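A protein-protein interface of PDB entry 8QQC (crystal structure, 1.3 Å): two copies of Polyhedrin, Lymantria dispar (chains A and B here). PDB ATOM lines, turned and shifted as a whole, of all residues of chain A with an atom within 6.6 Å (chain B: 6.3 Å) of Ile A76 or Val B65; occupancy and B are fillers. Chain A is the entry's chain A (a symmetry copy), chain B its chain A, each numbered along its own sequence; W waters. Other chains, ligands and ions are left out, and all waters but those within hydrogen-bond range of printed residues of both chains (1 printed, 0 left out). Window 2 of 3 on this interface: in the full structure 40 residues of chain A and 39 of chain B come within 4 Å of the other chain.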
ATOM      1  N   ALA A  75      20.657  12.062 -18.617  1.00  0.00           N
ATOM      2  CA  ALA A  75      19.982  10.800 -18.330  1.00  0.00           C
ATOM      3  C   ALA A  75      18.816  10.542 -19.276  1.00  0.00           C
ATOM      4  O   ALA A  75      18.480   9.392 -19.559  1.00  0.00           O
ATOM      5  CB  ALA A  75      19.500  10.764 -16.885  1.00  0.00           C
ATOM      6  N   ILE A  76      18.201  11.625 -19.761  1.00  0.00           N
ATOM      7  CA  ILE A  76      16.994  11.485 -20.571  1.00  0.00           C
ATOM      8  C   ILE A  76      17.283  10.755 -21.875  1.00  0.00           C
ATOM      9  O   ILE A  76      16.396  10.100 -22.433  1.00  0.00           O
ATOM     10  CB  ILE A  76      16.314  12.851 -20.793  1.00  0.00           C
ATOM     11  CG1 ILE A  76      14.929  12.664 -21.421  1.00  0.00           C
ATOM     12  CG2 ILE A  76      17.194  13.764 -21.657  1.00  0.00           C
ATOM     13  CD1 ILE A  76      13.920  12.001 -20.500  1.00  0.00           C
ATOM     14  N   TYR A  77      18.521  10.839 -22.375  1.00  0.00           N
ATOM     15  CA  TYR A  77      18.860  10.143 -23.613  1.00  0.00           C
ATOM     16  C   TYR A  77      18.665   8.641 -23.472  1.00  0.00           C
ATOM     17  O   TYR A  77      18.206   7.977 -24.411  1.00  0.00           O
ATOM     18  CB  TYR A  77      20.288  10.483 -24.046  1.00  0.00           C
ATOM     19  CG  TYR A  77      20.469  11.954 -24.327  1.00  0.00           C
ATOM     20  CD1 TYR A  77      20.284  12.459 -25.607  1.00  0.00           C
ATOM     21  CD2 TYR A  77      20.801  12.845 -23.313  1.00  0.00           C
ATOM     22  CE1 TYR A  77      20.438  13.806 -25.874  1.00  0.00           C
ATOM     23  CE2 TYR A  77      20.955  14.197 -23.571  1.00  0.00           C
ATOM     24  CZ  TYR A  77      20.772  14.670 -24.854  1.00  0.00           C
ATOM     25  OH  TYR A  77      20.925  16.012 -25.122  1.00  0.00           O
ATOM     26  N   TYR A  78      18.994   8.093 -22.297  1.00  0.00           N
ATOM     27  CA  TYR A  78      18.748   6.686 -22.004  1.00  0.00           C
ATOM     28  C   TYR A  78      17.311   6.454 -21.541  1.00  0.00           C
ATOM     29  O   TYR A  78      16.662   5.500 -21.985  1.00  0.00           O
ATOM     30  CB  TYR A  78      19.750   6.206 -20.948  1.00  0.00           C
ATOM     31  CG  TYR A  78      19.606   4.757 -20.541  1.00  0.00           C
ATOM     32  CD1 TYR A  78      20.261   3.752 -21.239  1.00  0.00           C
ATOM     33  CD2 TYR A  78      18.835   4.396 -19.444  1.00  0.00           C
ATOM     34  CE1 TYR A  78      20.138   2.424 -20.866  1.00  0.00           C
ATOM     35  CE2 TYR A  78      18.709   3.077 -19.065  1.00  0.00           C
ATOM     36  CZ  TYR A  78      19.361   2.096 -19.782  1.00  0.00           C
ATOM     37  OH  TYR A  78      19.237   0.779 -19.405  1.00  0.00           O
ATOM     38  N   ARG A  79      16.795   7.321 -20.661  1.00  0.00           N
ATOM     39  CA  ARG A  79      15.458   7.110 -20.110  1.00  0.00           C
ATOM     40  C   ARG A  79      14.396   7.077 -21.205  1.00  0.00           C
ATOM     41  O   ARG A  79      13.449   6.284 -21.135  1.00  0.00           O
ATOM     42  CB  ARG A  79      15.136   8.177 -19.065  1.00  0.00           C
ATOM     43  CG  ARG A  79      16.082   8.189 -17.875  1.00  0.00           C
ATOM     44  CD  ARG A  79      15.947   6.937 -17.040  1.00  0.00           C
ATOM     45  NE  ARG A  79      16.845   6.965 -15.890  1.00  0.00           N
ATOM     46  CZ  ARG A  79      16.479   7.290 -14.656  1.00  0.00           C
ATOM     47  NH1 ARG A  79      15.229   7.617 -14.367  1.00  0.00           N
ATOM     48  NH2 ARG A  79      17.391   7.281 -13.686  1.00  0.00           N
ATOM     49  N   GLU A  80      14.542   7.914 -22.235  1.00  0.00           N
ATOM     50  CA  GLU A  80      13.547   7.912 -23.305  1.00  0.00           C
ATOM     51  C   GLU A  80      13.518   6.573 -24.030  1.00  0.00           C
ATOM     52  O   GLU A  80      12.465   6.162 -24.529  1.00  0.00           O
ATOM     53  CB  GLU A  80      13.803   9.051 -24.293  1.00  0.00           C
ATOM     54  CG  GLU A  80      12.573   9.436 -25.120  1.00  0.00           C
ATOM     55  CD  GLU A  80      11.621  10.357 -24.375  1.00  0.00           C
ATOM     56  OE1 GLU A  80      11.770  10.504 -23.146  1.00  0.00           O
ATOM     57  OE2 GLU A  80      10.718  10.933 -25.018  1.00  0.00           O
ATOM     58  N   GLY A  81      14.657   5.877 -24.087  1.00  0.00           N
ATOM     59  CA  GLY A  81      14.715   4.574 -24.728  1.00  0.00           C
ATOM     60  C   GLY A  81      14.044   3.461 -23.955  1.00  0.00           C
ATOM     61  O   GLY A  81      13.660   2.451 -24.553  1.00  0.00           O
ATOM     62  N   THR A  83      11.380   4.366 -22.048  1.00  0.00           N
ATOM     63  CA  THR A  83      10.021   4.881 -21.964  1.00  0.00           C
ATOM     64  C   THR A  83       9.164   4.423 -23.139  1.00  0.00           C
ATOM     65  O   THR A  83       8.043   3.950 -22.943  1.00  0.00           O
ATOM     66  CB  THR A  83      10.040   6.409 -21.885  1.00  0.00           C
ATOM     67  OG1 THR A  83      10.726   6.817 -20.694  1.00  0.00           O
ATOM     68  CG2 THR A  83       8.621   6.963 -21.886  1.00  0.00           C
ATOM     69  N   ALA A  87      12.755   4.789 -28.870  1.00  0.00           N
ATOM     70  CA  ALA A  87      12.707   6.234 -28.695  1.00  0.00           C
ATOM     71  C   ALA A  87      13.955   6.796 -28.029  1.00  0.00           C
ATOM     72  O   ALA A  87      13.990   7.989 -27.715  1.00  0.00           O
ATOM     73  CB  ALA A  87      11.461   6.637 -27.904  1.00  0.00           C
ATOM     74  N   GLY A  88      14.982   5.975 -27.815  1.00  0.00           N
ATOM     75  CA  GLY A  88      16.161   6.450 -27.127  1.00  0.00           C
ATOM     76  C   GLY A  88      17.135   7.177 -28.030  1.00  0.00           C
ATOM     77  O   GLY A  88      17.077   7.105 -29.254  1.00  0.00           O
ATOM     78  N   ASP A  89      18.047   7.904 -27.390  1.00  0.00           N
ATOM     79  CA  ASP A  89      19.145   8.578 -28.074  1.00  0.00           C
ATOM     80  C   ASP A  89      20.435   8.359 -27.292  1.00  0.00           C
ATOM     81  O   ASP A  89      21.183   9.290 -26.989  1.00  0.00           O
ATOM     82  CB  ASP A  89      18.834  10.061 -28.267  1.00  0.00           C
ATOM     83  CG  ASP A  89      19.791  10.740 -29.225  1.00  0.00           C
ATOM     84  OD1 ASP A  89      20.571  10.037 -29.902  1.00  0.00           O
ATOM     85  OD2 ASP A  89      19.755  11.984 -29.299  1.00  0.00           O
ATOM     86  N   ILE B  62       7.688  21.446 -12.313  1.00  0.00           N
ATOM     87  CA  ILE B  62       8.588  22.195 -13.177  1.00  0.00           C
ATOM     88  C   ILE B  62       9.305  21.237 -14.125  1.00  0.00           C
ATOM     89  O   ILE B  62       9.352  20.027 -13.910  1.00  0.00           O
ATOM     90  CB  ILE B  62       9.578  23.061 -12.374  1.00  0.00           C
ATOM     91  CG1 ILE B  62      10.505  22.180 -11.533  1.00  0.00           C
ATOM     92  CG2 ILE B  62       8.819  24.030 -11.490  1.00  0.00           C
ATOM     93  CD1 ILE B  62      11.606  22.964 -10.828  1.00  0.00           C
ATOM     94  N   ASN B  63       9.859  21.790 -15.201  1.00  0.00           N
ATOM     95  CA  ASN B  63      10.571  20.992 -16.195  1.00  0.00           C
ATOM     96  C   ASN B  63      11.914  20.571 -15.605  1.00  0.00           C
ATOM     97  O   ASN B  63      12.774  21.421 -15.351  1.00  0.00           O
ATOM     98  CB  ASN B  63      10.783  21.848 -17.440  1.00  0.00           C
ATOM     99  CG  ASN B  63      11.368  21.072 -18.610  1.00  0.00           C
ATOM    100  OD1 ASN B  63      12.026  20.042 -18.436  1.00  0.00           O
ATOM    101  ND2 ASN B  63      11.140  21.579 -19.818  1.00  0.00           N
ATOM    102  N   ASN B  64      12.112  19.267 -15.400  1.00  0.00           N
ATOM    103  CA  ASN B  64      13.342  18.770 -14.791  1.00  0.00           C
ATOM    104  C   ASN B  64      14.337  18.240 -15.814  1.00  0.00           C
ATOM    105  O   ASN B  64      15.354  17.657 -15.427  1.00  0.00           O
ATOM    106  CB  ASN B  64      13.057  17.680 -13.755  1.00  0.00           C
ATOM    107  CG  ASN B  64      12.349  16.479 -14.346  1.00  0.00           C
ATOM    108  OD1 ASN B  64      11.764  16.553 -15.428  1.00  0.00           O
ATOM    109  ND2 ASN B  64      12.418  15.350 -13.643  1.00  0.00           N
ATOM    110  N   VAL B  65      14.064  18.405 -17.104  1.00  0.00           N
ATOM    111  CA  VAL B  65      14.986  18.009 -18.161  1.00  0.00           C
ATOM    112  C   VAL B  65      15.671  19.218 -18.783  1.00  0.00           C
ATOM    113  O   VAL B  65      16.898  19.273 -18.865  1.00  0.00           O
ATOM    114  CB  VAL B  65      14.293  17.137 -19.232  1.00  0.00           C
ATOM    115  CG1 VAL B  65      15.253  16.842 -20.380  1.00  0.00           C
ATOM    116  CG2 VAL B  65      13.791  15.847 -18.614  1.00  0.00           C
ATOM    117  N   ASN B  66      14.891  20.195 -19.233  1.00  0.00           N
ATOM    118  CA  ASN B  66      15.434  21.474 -19.683  1.00  0.00           C
ATOM    119  C   ASN B  66      15.315  22.390 -18.469  1.00  0.00           C
ATOM    120  O   ASN B  66      14.315  23.086 -18.284  1.00  0.00           O
ATOM    121  CB  ASN B  66      14.664  21.996 -20.889  1.00  0.00           C
ATOM    122  CG  ASN B  66      15.283  23.249 -21.479  1.00  0.00           C
ATOM    123  OD1 ASN B  66      16.402  23.629 -21.125  1.00  0.00           O
ATOM    124  ND2 ASN B  66      14.563  23.892 -22.394  1.00  0.00           N
ATOM    125  N   ARG B  67      16.341  22.361 -17.625  1.00  0.00           N
ATOM    126  CA  ARG B  67      16.272  22.966 -16.295  1.00  0.00           C
ATOM    127  C   ARG B  67      16.894  24.360 -16.232  1.00  0.00           C
ATOM    128  O   ARG B  67      17.017  25.047 -17.248  1.00  0.00           O
ATOM    129  CB  ARG B  67      16.942  22.047 -15.266  1.00  0.00           C
ATOM    130  N   TRP B 208       7.425  10.938 -16.594  1.00  0.00           N
ATOM    131  CA  TRP B 208       8.229  10.878 -17.805  1.00  0.00           C
ATOM    132  C   TRP B 208       8.314  12.279 -18.393  1.00  0.00           C
ATOM    133  O   TRP B 208       7.594  13.197 -17.985  1.00  0.00           O
ATOM    134  CB  TRP B 208       7.599   9.972 -18.869  1.00  0.00           C
ATOM    135  CG  TRP B 208       7.227   8.582 -18.440  1.00  0.00           C
ATOM    136  CD1 TRP B 208       7.973   7.453 -18.600  1.00  0.00           C
ATOM    137  CD2 TRP B 208       5.990   8.164 -17.849  1.00  0.00           C
ATOM    138  NE1 TRP B 208       7.292   6.360 -18.122  1.00  0.00           N
ATOM    139  CE2 TRP B 208       6.072   6.771 -17.653  1.00  0.00           C
ATOM    140  CE3 TRP B 208       4.831   8.834 -17.444  1.00  0.00           C
ATOM    141  CZ2 TRP B 208       5.040   6.035 -17.074  1.00  0.00           C
ATOM    142  CZ3 TRP B 208       3.804   8.099 -16.872  1.00  0.00           C
ATOM    143  CH2 TRP B 208       3.917   6.713 -16.696  1.00  0.00           C
ATOM    144  N   TRP B 209       9.183  12.434 -19.392  1.00  0.00           N
ATOM    145  CA  TRP B 209       9.315  13.697 -20.105  1.00  0.00           C
ATOM    146  C   TRP B 209       9.501  13.405 -21.583  1.00  0.00           C
ATOM    147  O   TRP B 209      10.140  12.416 -21.953  1.00  0.00           O
ATOM    148  CB  TRP B 209      10.514  14.490 -19.576  1.00  0.00           C
ATOM    149  CG  TRP B 209      10.834  15.770 -20.319  1.00  0.00           C
ATOM    150  CD1 TRP B 209      10.448  17.034 -19.970  1.00  0.00           C
ATOM    151  CD2 TRP B 209      11.638  15.912 -21.503  1.00  0.00           C
ATOM    152  NE1 TRP B 209      10.946  17.949 -20.867  1.00  0.00           N
ATOM    153  CE2 TRP B 209      11.681  17.288 -21.817  1.00  0.00           C
ATOM    154  CE3 TRP B 209      12.320  15.011 -22.331  1.00  0.00           C
ATOM    155  CZ2 TRP B 209      12.382  17.783 -22.924  1.00  0.00           C
ATOM    156  CZ3 TRP B 209      13.008  15.503 -23.435  1.00  0.00           C
ATOM    157  CH2 TRP B 209      13.033  16.875 -23.719  1.00  0.00           C
ATOM    158  N   PHE B 210       8.943  14.282 -22.424  1.00  0.00           N
ATOM    159  CA  PHE B 210       8.969  14.121 -23.876  1.00  0.00           C
ATOM    160  C   PHE B 210       9.292  15.451 -24.539  1.00  0.00           C
ATOM    161  O   PHE B 210       8.836  16.505 -24.074  1.00  0.00           O
ATOM    162  CB  PHE B 210       7.633  13.586 -24.411  1.00  0.00           C
ATOM    163  CG  PHE B 210       7.184  12.328 -23.731  1.00  0.00           C
ATOM    164  CD1 PHE B 210       7.597  11.097 -24.197  1.00  0.00           C
ATOM    165  CD2 PHE B 210       6.392  12.380 -22.591  1.00  0.00           C
ATOM    166  CE1 PHE B 210       7.207   9.937 -23.559  1.00  0.00           C
ATOM    167  CE2 PHE B 210       6.003  11.220 -21.945  1.00  0.00           C
ATOM    168  CZ  PHE B 210       6.413   9.999 -22.432  1.00  0.00           C
HETATM  169  O   HOH W   1      10.892   9.628 -20.176  1.00  0.00           O
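The side-chain carboxylate (OE1) of Glu A80 sits close to the backbone carbonyl oxygen (O) of Trp B209.
CG1 of Val B65 touches CG2 of Ile A76, at 3.9 Å.
CG1 of Ile A76 touches CE3 of Trp B209 (3.6 Å).
Phe B210 touches Glu A80 (CD1 to OE2, 3.2 Å).
Trp B208 touches Thr A83 (CD1 to CG2, 3.4 Å).
CE1 of Phe B210 touches CG2 of Thr A83, 3.7 Å away.
Of the printed residues of chain B, Glu A80 touches Trp B209 (2.8 Å) and Phe B210 (3.2 Å).
Of the printed residues of chain B, Thr A83 touches Trp B208 (3.4 Å) and Phe B210 (3.7 Å).
Asp A89 touches none of the printed residues of chain B.
Printed residues of chain A within 4 Å of Val B65: Ile A76.
Of the printed residues of chain A, Trp B208 touches Thr A83 (3.4 Å).
Of the printed residues of chain A, Trp B209 touches Ile A76 (3.6 Å) and Glu A80 (2.8 Å).
Of the printed residues of chain A, Phe B210 touches Glu A80 and Thr A83.
The nearest residue of chain B that does not touch Ile A76 is Phe B210 (5.8 Å).
Hydrophobic or aromatic side chains of chain B within 4 Å of the printed part of chain A: Val B65, Trp B208, Trp B209 and Phe B210.
Hydrophobic or aromatic side chains of chain A within 4 Å of the printed part of chain B: Ile A76.
No position is printed for both chains.
Of the 6 pairs that touch across the chains among the printed residues, none has its exchanged pair printed and touching as well.
OD1 of Asn B63 lies within hydrogen-bond range of NE1 of Trp B209 (3.4 Å).
N of Val B65 lies within hydrogen-bond range of OD1 of Asn B63 (2.9 Å).
The backbone carbonyl oxygen of Arg A79 lies within hydrogen-bond range of the side-chain hydroxyl of Thr A83 (2.8 Å).
Water W1 lies within hydrogen-bond range of the side-chain hydroxyl (OG1) of Thr A83 (2.9 Å), the side-chain carboxylate (OE1) of Glu A80 (3.2 Å) and the backbone NH (N) of Trp B209 (3.4 Å).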
